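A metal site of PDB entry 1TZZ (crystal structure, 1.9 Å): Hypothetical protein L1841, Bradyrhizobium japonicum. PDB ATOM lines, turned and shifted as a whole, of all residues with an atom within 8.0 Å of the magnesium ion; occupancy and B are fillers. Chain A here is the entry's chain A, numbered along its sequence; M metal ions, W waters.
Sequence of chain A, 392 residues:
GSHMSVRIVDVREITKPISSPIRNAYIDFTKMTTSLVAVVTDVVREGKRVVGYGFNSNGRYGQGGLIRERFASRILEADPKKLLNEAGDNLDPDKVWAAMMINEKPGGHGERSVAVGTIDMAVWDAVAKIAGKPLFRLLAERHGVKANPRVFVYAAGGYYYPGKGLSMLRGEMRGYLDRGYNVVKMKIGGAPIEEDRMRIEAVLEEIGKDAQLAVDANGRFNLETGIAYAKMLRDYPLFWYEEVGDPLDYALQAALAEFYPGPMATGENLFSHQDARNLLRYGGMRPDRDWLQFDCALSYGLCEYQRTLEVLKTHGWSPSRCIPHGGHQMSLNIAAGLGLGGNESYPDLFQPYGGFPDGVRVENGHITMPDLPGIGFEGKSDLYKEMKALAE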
ATOM      1  N   TYR A 154       0.667  30.637 -24.280  1.00  0.00           N
ATOM      2  CA  TYR A 154       0.876  29.522 -25.204  1.00  0.00           C
ATOM      3  C   TYR A 154      -0.481  28.977 -25.625  1.00  0.00           C
ATOM      4  O   TYR A 154      -1.463  29.124 -24.903  1.00  0.00           O
ATOM      5  CB  TYR A 154       1.729  28.408 -24.562  1.00  0.00           C
ATOM      6  CG  TYR A 154       1.014  27.532 -23.545  1.00  0.00           C
ATOM      7  CD1 TYR A 154       0.360  26.365 -23.949  1.00  0.00           C
ATOM      8  CD2 TYR A 154       0.983  27.871 -22.192  1.00  0.00           C
ATOM      9  CE1 TYR A 154      -0.305  25.548 -23.025  1.00  0.00           C
ATOM     10  CE2 TYR A 154       0.320  27.064 -21.267  1.00  0.00           C
ATOM     11  CZ  TYR A 154      -0.326  25.909 -21.688  1.00  0.00           C
ATOM     12  OH  TYR A 154      -1.022  25.131 -20.768  1.00  0.00           O
ATOM     13  N   ALA A 156      -3.044  26.011 -26.264  1.00  0.00           N
ATOM     14  CA  ALA A 156      -3.331  24.646 -25.841  1.00  0.00           C
ATOM     15  C   ALA A 156      -4.371  23.994 -26.744  1.00  0.00           C
ATOM     16  O   ALA A 156      -5.475  24.534 -26.923  1.00  0.00           O
ATOM     17  CB  ALA A 156      -3.816  24.627 -24.399  1.00  0.00           C
ATOM     18  N   LYS A 185       0.790  23.329 -27.361  1.00  0.00           N
ATOM     19  CA  LYS A 185       0.731  22.091 -26.577  1.00  0.00           C
ATOM     20  C   LYS A 185      -0.259  21.123 -27.215  1.00  0.00           C
ATOM     21  O   LYS A 185      -1.317  21.543 -27.690  1.00  0.00           O
ATOM     22  CB  LYS A 185       0.304  22.383 -25.141  1.00  0.00           C
ATOM     23  CG  LYS A 185       0.354  21.155 -24.221  1.00  0.00           C
ATOM     24  CD  LYS A 185       0.028  21.514 -22.770  1.00  0.00           C
ATOM     25  CE  LYS A 185      -1.432  21.890 -22.587  1.00  0.00           C
ATOM     26  NZ  LYS A 185      -1.721  22.326 -21.199  1.00  0.00           N
ATOM     27  N   MET A 186       0.074  19.837 -27.197  1.00  0.00           N
ATOM     28  CA  MET A 186      -0.797  18.809 -27.779  1.00  0.00           C
ATOM     29  C   MET A 186      -1.026  17.708 -26.741  1.00  0.00           C
ATOM     30  O   MET A 186      -0.287  17.600 -25.759  1.00  0.00           O
ATOM     31  CB  MET A 186      -0.144  18.204 -29.016  1.00  0.00           C
ATOM     32  CG  MET A 186       1.163  17.473 -28.753  1.00  0.00           C
ATOM     33  SD  MET A 186       1.990  16.895 -30.285  1.00  0.00           S
ATOM     34  CE  MET A 186       1.049  15.375 -30.625  1.00  0.00           C
ATOM     35  N   LYS A 187      -2.039  16.885 -26.969  1.00  0.00           N
ATOM     36  CA  LYS A 187      -2.322  15.791 -26.060  1.00  0.00           C
ATOM     37  C   LYS A 187      -1.605  14.519 -26.479  1.00  0.00           C
ATOM     38  O   LYS A 187      -1.355  14.303 -27.661  1.00  0.00           O
ATOM     39  CB  LYS A 187      -3.824  15.526 -26.025  1.00  0.00           C
ATOM     40  CG  LYS A 187      -4.647  16.652 -25.424  1.00  0.00           C
ATOM     41  CD  LYS A 187      -6.090  16.214 -25.218  1.00  0.00           C
ATOM     42  CE  LYS A 187      -6.825  17.148 -24.274  1.00  0.00           C
ATOM     43  NZ  LYS A 187      -8.194  16.634 -23.932  1.00  0.00           N
ATOM     44  N   VAL A 215       3.717  18.673 -24.481  1.00  0.00           N
ATOM     45  CA  VAL A 215       2.807  17.547 -24.564  1.00  0.00           C
ATOM     46  C   VAL A 215       2.117  17.365 -23.219  1.00  0.00           C
ATOM     47  O   VAL A 215       2.703  17.636 -22.167  1.00  0.00           O
ATOM     48  CB  VAL A 215       3.530  16.246 -24.953  1.00  0.00           C
ATOM     49  CG1 VAL A 215       4.155  16.397 -26.330  1.00  0.00           C
ATOM     50  CG2 VAL A 215       4.584  15.905 -23.915  1.00  0.00           C
ATOM     51  N   ASP A 216       0.867  16.917 -23.254  1.00  0.00           N
ATOM     52  CA  ASP A 216       0.054  16.741 -22.057  1.00  0.00           C
ATOM     53  C   ASP A 216      -0.594  15.363 -21.975  1.00  0.00           C
ATOM     54  O   ASP A 216      -1.402  14.993 -22.840  1.00  0.00           O
ATOM     55  CB  ASP A 216      -1.032  17.812 -22.079  1.00  0.00           C
ATOM     56  CG  ASP A 216      -1.764  17.932 -20.780  1.00  0.00           C
ATOM     57  OD1 ASP A 216      -1.559  17.095 -19.861  1.00  0.00           O
ATOM     58  OD2 ASP A 216      -2.551  18.876 -20.685  1.00  0.00           O
ATOM     59  N   ALA A 217      -0.256  14.607 -20.936  1.00  0.00           N
ATOM     60  CA  ALA A 217      -0.789  13.265 -20.755  1.00  0.00           C
ATOM     61  C   ALA A 217      -2.109  13.242 -19.981  1.00  0.00           C
ATOM     62  O   ALA A 217      -2.715  12.184 -19.825  1.00  0.00           O
ATOM     63  CB  ALA A 217       0.236  12.391 -20.056  1.00  0.00           C
ATOM     64  N   ASN A 218      -2.535  14.398 -19.487  1.00  0.00           N
ATOM     65  CA  ASN A 218      -3.786  14.503 -18.760  1.00  0.00           C
ATOM     66  C   ASN A 218      -3.937  13.525 -17.592  1.00  0.00           C
ATOM     67  O   ASN A 218      -5.034  13.070 -17.293  1.00  0.00           O
ATOM     68  CB  ASN A 218      -4.964  14.325 -19.723  1.00  0.00           C
ATOM     69  CG  ASN A 218      -5.032  15.433 -20.757  1.00  0.00           C
ATOM     70  OD1 ASN A 218      -5.315  16.587 -20.423  1.00  0.00           O
ATOM     71  ND2 ASN A 218      -4.778  15.095 -22.016  1.00  0.00           N
ATOM     72  N   GLY A 219      -2.815  13.213 -16.939  1.00  0.00           N
ATOM     73  CA  GLY A 219      -2.822  12.318 -15.782  1.00  0.00           C
ATOM     74  C   GLY A 219      -3.172  10.873 -16.046  1.00  0.00           C
ATOM     75  O   GLY A 219      -3.508  10.124 -15.127  1.00  0.00           O
ATOM     76  N   TRP A 240       7.703  21.128 -22.538  1.00  0.00           N
ATOM     77  CA  TRP A 240       7.424  20.446 -21.282  1.00  0.00           C
ATOM     78  C   TRP A 240       6.566  19.200 -21.460  1.00  0.00           C
ATOM     79  O   TRP A 240       5.906  19.025 -22.488  1.00  0.00           O
ATOM     80  CB  TRP A 240       6.780  21.378 -20.229  1.00  0.00           C
ATOM     81  CG  TRP A 240       5.342  21.741 -20.429  1.00  0.00           C
ATOM     82  CD1 TRP A 240       4.279  20.882 -20.623  1.00  0.00           C
ATOM     83  CD2 TRP A 240       4.775  23.050 -20.330  1.00  0.00           C
ATOM     84  NE1 TRP A 240       3.101  21.597 -20.643  1.00  0.00           N
ATOM     85  CE2 TRP A 240       3.374  22.929 -20.458  1.00  0.00           C
ATOM     86  CE3 TRP A 240       5.326  24.323 -20.128  1.00  0.00           C
ATOM     87  CZ2 TRP A 240       2.509  24.024 -20.395  1.00  0.00           C
ATOM     88  CZ3 TRP A 240       4.454  25.430 -20.066  1.00  0.00           C
ATOM     89  CH2 TRP A 240       3.072  25.263 -20.194  1.00  0.00           C
ATOM     90  N   GLU A 242       3.632  17.375 -19.512  1.00  0.00           N
ATOM     91  CA  GLU A 242       2.614  17.696 -18.516  1.00  0.00           C
ATOM     92  C   GLU A 242       1.716  16.595 -17.943  1.00  0.00           C
ATOM     93  O   GLU A 242       1.257  15.704 -18.655  1.00  0.00           O
ATOM     94  CB  GLU A 242       1.736  18.823 -19.079  1.00  0.00           C
ATOM     95  CG  GLU A 242       0.671  19.352 -18.131  1.00  0.00           C
ATOM     96  CD  GLU A 242      -0.164  20.452 -18.771  1.00  0.00           C
ATOM     97  OE1 GLU A 242       0.366  21.210 -19.603  1.00  0.00           O
ATOM     98  OE2 GLU A 242      -1.341  20.573 -18.429  1.00  0.00           O
ATOM     99  N   GLU A 243       1.468  16.733 -16.635  1.00  0.00           N
ATOM    100  CA  GLU A 243       0.636  15.833 -15.830  1.00  0.00           C
ATOM    101  C   GLU A 243       0.705  14.373 -16.263  1.00  0.00           C
ATOM    102  O   GLU A 243      -0.248  13.805 -16.796  1.00  0.00           O
ATOM    103  CB  GLU A 243      -0.819  16.330 -15.840  1.00  0.00           C
ATOM    104  CG  GLU A 243      -1.674  15.711 -14.733  1.00  0.00           C
ATOM    105  CD  GLU A 243      -3.078  16.281 -14.646  1.00  0.00           C
ATOM    106  OE1 GLU A 243      -3.702  16.502 -15.708  1.00  0.00           O
ATOM    107  OE2 GLU A 243      -3.574  16.483 -13.523  1.00  0.00           O
ATOM    108  N   ALA A 265       5.487  19.635 -16.055  1.00  0.00           N
ATOM    109  CA  ALA A 265       4.468  20.515 -15.509  1.00  0.00           C
ATOM    110  C   ALA A 265       3.289  19.742 -14.929  1.00  0.00           C
ATOM    111  O   ALA A 265       3.021  18.626 -15.368  1.00  0.00           O
ATOM    112  CB  ALA A 265       3.969  21.470 -16.619  1.00  0.00           C
ATOM    113  N   THR A 266       2.608  20.332 -13.952  1.00  0.00           N
ATOM    114  CA  THR A 266       1.435  19.701 -13.363  1.00  0.00           C
ATOM    115  C   THR A 266       0.756  20.668 -12.388  1.00  0.00           C
ATOM    116  O   THR A 266       1.257  21.773 -12.180  1.00  0.00           O
ATOM    117  CB  THR A 266       1.801  18.398 -12.607  1.00  0.00           C
ATOM    118  OG1 THR A 266       0.597  17.676 -12.310  1.00  0.00           O
ATOM    119  CG2 THR A 266       2.531  18.711 -11.301  1.00  0.00           C
ATOM    120  N   GLY A 267      -0.386  20.267 -11.833  1.00  0.00           N
ATOM    121  CA  GLY A 267      -1.056  21.116 -10.861  1.00  0.00           C
ATOM    122  C   GLY A 267      -2.439  21.646 -11.181  1.00  0.00           C
ATOM    123  O   GLY A 267      -3.130  22.138 -10.282  1.00  0.00           O
ATOM    124  N   GLU A 268      -2.862  21.554 -12.437  1.00  0.00           N
ATOM    125  CA  GLU A 268      -4.185  22.068 -12.806  1.00  0.00           C
ATOM    126  C   GLU A 268      -5.292  21.384 -12.017  1.00  0.00           C
ATOM    127  O   GLU A 268      -6.369  21.950 -11.831  1.00  0.00           O
ATOM    128  CB  GLU A 268      -4.438  21.879 -14.310  1.00  0.00           C
ATOM    129  CG  GLU A 268      -5.033  20.526 -14.691  1.00  0.00           C
ATOM    130  CD  GLU A 268      -5.125  20.372 -16.199  1.00  0.00           C
ATOM    131  OE1 GLU A 268      -4.063  20.390 -16.836  1.00  0.00           O
ATOM    132  OE2 GLU A 268      -6.251  20.236 -16.745  1.00  0.00           O
ATOM    133  N   ASN A 269      -5.038  20.154 -11.554  1.00  0.00           N
ATOM    134  CA  ASN A 269      -6.034  19.427 -10.793  1.00  0.00           C
ATOM    135  C   ASN A 269      -5.783  19.353  -9.281  1.00  0.00           C
ATOM    136  O   ASN A 269      -6.248  18.433  -8.609  1.00  0.00           O
ATOM    137  CB  ASN A 269      -6.232  18.028 -11.374  1.00  0.00           C
ATOM    138  CG  ASN A 269      -6.938  18.055 -12.734  1.00  0.00           C
ATOM    139  OD1 ASN A 269      -7.998  18.663 -12.882  1.00  0.00           O
ATOM    140  ND2 ASN A 269      -6.334  17.404 -13.730  1.00  0.00           N
ATOM    141  N   GLN A 293       0.818  24.572 -12.625  1.00  0.00           N
ATOM    142  CA  GLN A 293      -0.395  25.003 -13.288  1.00  0.00           C
ATOM    143  C   GLN A 293      -1.682  25.163 -12.480  1.00  0.00           C
ATOM    144  O   GLN A 293      -2.770  25.073 -13.041  1.00  0.00           O
ATOM    145  CB  GLN A 293      -0.632  24.080 -14.487  1.00  0.00           C
ATOM    146  CG  GLN A 293       0.619  23.995 -15.367  1.00  0.00           C
ATOM    147  CD  GLN A 293       0.551  22.896 -16.407  1.00  0.00           C
ATOM    148  OE1 GLN A 293       0.475  21.717 -16.069  1.00  0.00           O
ATOM    149  NE2 GLN A 293       0.573  23.265 -17.680  1.00  0.00           N
ATOM    150  N   HIS A 325      -3.604  27.186 -15.167  1.00  0.00           N
ATOM    151  CA  HIS A 325      -4.535  26.587 -16.106  1.00  0.00           C
ATOM    152  C   HIS A 325      -5.730  27.554 -16.108  1.00  0.00           C
ATOM    153  O   HIS A 325      -5.940  28.270 -15.122  1.00  0.00           O
ATOM    154  CB  HIS A 325      -4.937  25.191 -15.593  1.00  0.00           C
ATOM    155  CG  HIS A 325      -6.224  24.658 -16.161  1.00  0.00           C
ATOM    156  ND1 HIS A 325      -7.456  25.077 -15.723  1.00  0.00           N
ATOM    157  CD2 HIS A 325      -6.451  23.715 -17.109  1.00  0.00           C
ATOM    158  CE1 HIS A 325      -8.404  24.403 -16.363  1.00  0.00           C
ATOM    159  NE2 HIS A 325      -7.813  23.569 -17.208  1.00  0.00           N
ATOM    160  N   GLU A 344      -2.143  30.312 -20.410  1.00  0.00           N
ATOM    161  CA  GLU A 344      -2.475  29.386 -21.478  1.00  0.00           C
ATOM    162  C   GLU A 344      -3.707  29.953 -22.170  1.00  0.00           C
ATOM    163  O   GLU A 344      -4.468  30.730 -21.577  1.00  0.00           O
ATOM    164  CB  GLU A 344      -2.799  27.996 -20.933  1.00  0.00           C
ATOM    165  CG  GLU A 344      -4.059  27.886 -20.112  1.00  0.00           C
ATOM    166  CD  GLU A 344      -4.300  26.468 -19.631  1.00  0.00           C
ATOM    167  OE1 GLU A 344      -3.338  25.686 -19.595  1.00  0.00           O
ATOM    168  OE2 GLU A 344      -5.451  26.138 -19.268  1.00  0.00           O
ATOM    169  N   TYR A 346      -6.862  28.854 -25.266  1.00  0.00           N
ATOM    170  CA  TYR A 346      -7.497  27.817 -26.088  1.00  0.00           C
ATOM    171  C   TYR A 346      -8.136  28.566 -27.262  1.00  0.00           C
ATOM    172  O   TYR A 346      -9.306  28.937 -27.189  1.00  0.00           O
ATOM    173  CB  TYR A 346      -8.583  27.104 -25.287  1.00  0.00           C
ATOM    174  CG  TYR A 346      -8.123  26.467 -23.989  1.00  0.00           C
ATOM    175  CD1 TYR A 346      -7.552  25.188 -23.979  1.00  0.00           C
ATOM    176  CD2 TYR A 346      -8.299  27.119 -22.772  1.00  0.00           C
ATOM    177  CE1 TYR A 346      -7.181  24.570 -22.777  1.00  0.00           C
ATOM    178  CE2 TYR A 346      -7.937  26.513 -21.561  1.00  0.00           C
ATOM    179  CZ  TYR A 346      -7.380  25.241 -21.574  1.00  0.00           C
ATOM    180  OH  TYR A 346      -7.037  24.623 -20.390  1.00  0.00           O
HETATM  181 MG    MG M   1      -3.212  19.725 -18.759  1.00  0.00          MG
HETATM  182  O   HOH W   1      -5.247  19.300 -19.235  1.00  0.00           O
HETATM  183  O   HOH W   2      -3.042  17.987 -17.789  1.00  0.00           O
HETATM  184  O   HOH W   3      -3.743  21.610 -19.557  1.00  0.00           O
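The side-chain carboxylate (OD1) of Asp 216 lies within hydrogen-bond range of the backbone NH (N) of Asn 218, at 2.9 Å.
The backbone carbonyl oxygen (O) of Glu 242 sits at hydrogen-bond distance from the backbone NH (N) of Ala 217 (2.9 Å).
NZ of Lys 185 lies within hydrogen-bond range of OH of Tyr 154, at 2.9 Å.
The side-chain carboxylate (OE1) of Glu 242 is in salt-bridge range of the side-chain amino group (NZ) of Lys 185, 2.9 Å away.
OE1 of Glu 242 lies within hydrogen-bond range of NE2 of Gln 293, at 2.8 Å.
The backbone NH (N) of Glu 242 is in hydrogen-bond range of the backbone carbonyl oxygen (O) of Val 215, 2.8 Å away.
The backbone NH of Asp 216 is in hydrogen-bond range of the backbone carbonyl oxygen of Met 186, at 2.8 Å.
The side-chain amino group of Lys 185 lies close to the side-chain carboxylate of Asp 216, at 3.6 Å.
Water W2 binds the magnesium ion (2.0 Å).
The magnesium ion is bound by OE2 of Glu 242 (2.1 Å).
Water W3 is bound to the magnesium ion (2.1 Å).
Water W1 binds the magnesium ion, at 2.1 Å.
The magnesium ion is bound by OE1 of Glu 268.
The side-chain carboxylate (OD2) of Asp 216 binds the magnesium ion (2.2 Å).
Merely in contact with the magnesium ion: Lys 185 (3.9 Å).
Four residues have an atom within 4 Å of the magnesium ion: Lys 185, Asp 216, Glu 242 and Glu 268.
The nearest printed residue that does not touch the magnesium ion is Asn 218 (4.1 Å).
Water W1 lies within hydrogen-bond range of the side-chain carboxylate of Glu 268 (2.8 Å) and the side-chain amide oxygen of Asn 218 (3.0 Å).
Water W2 lies within hydrogen-bond range of the side-chain carboxylate of Glu 243 (2.6 Å) and the side-chain carboxylate of Asp 216 (2.7 Å).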
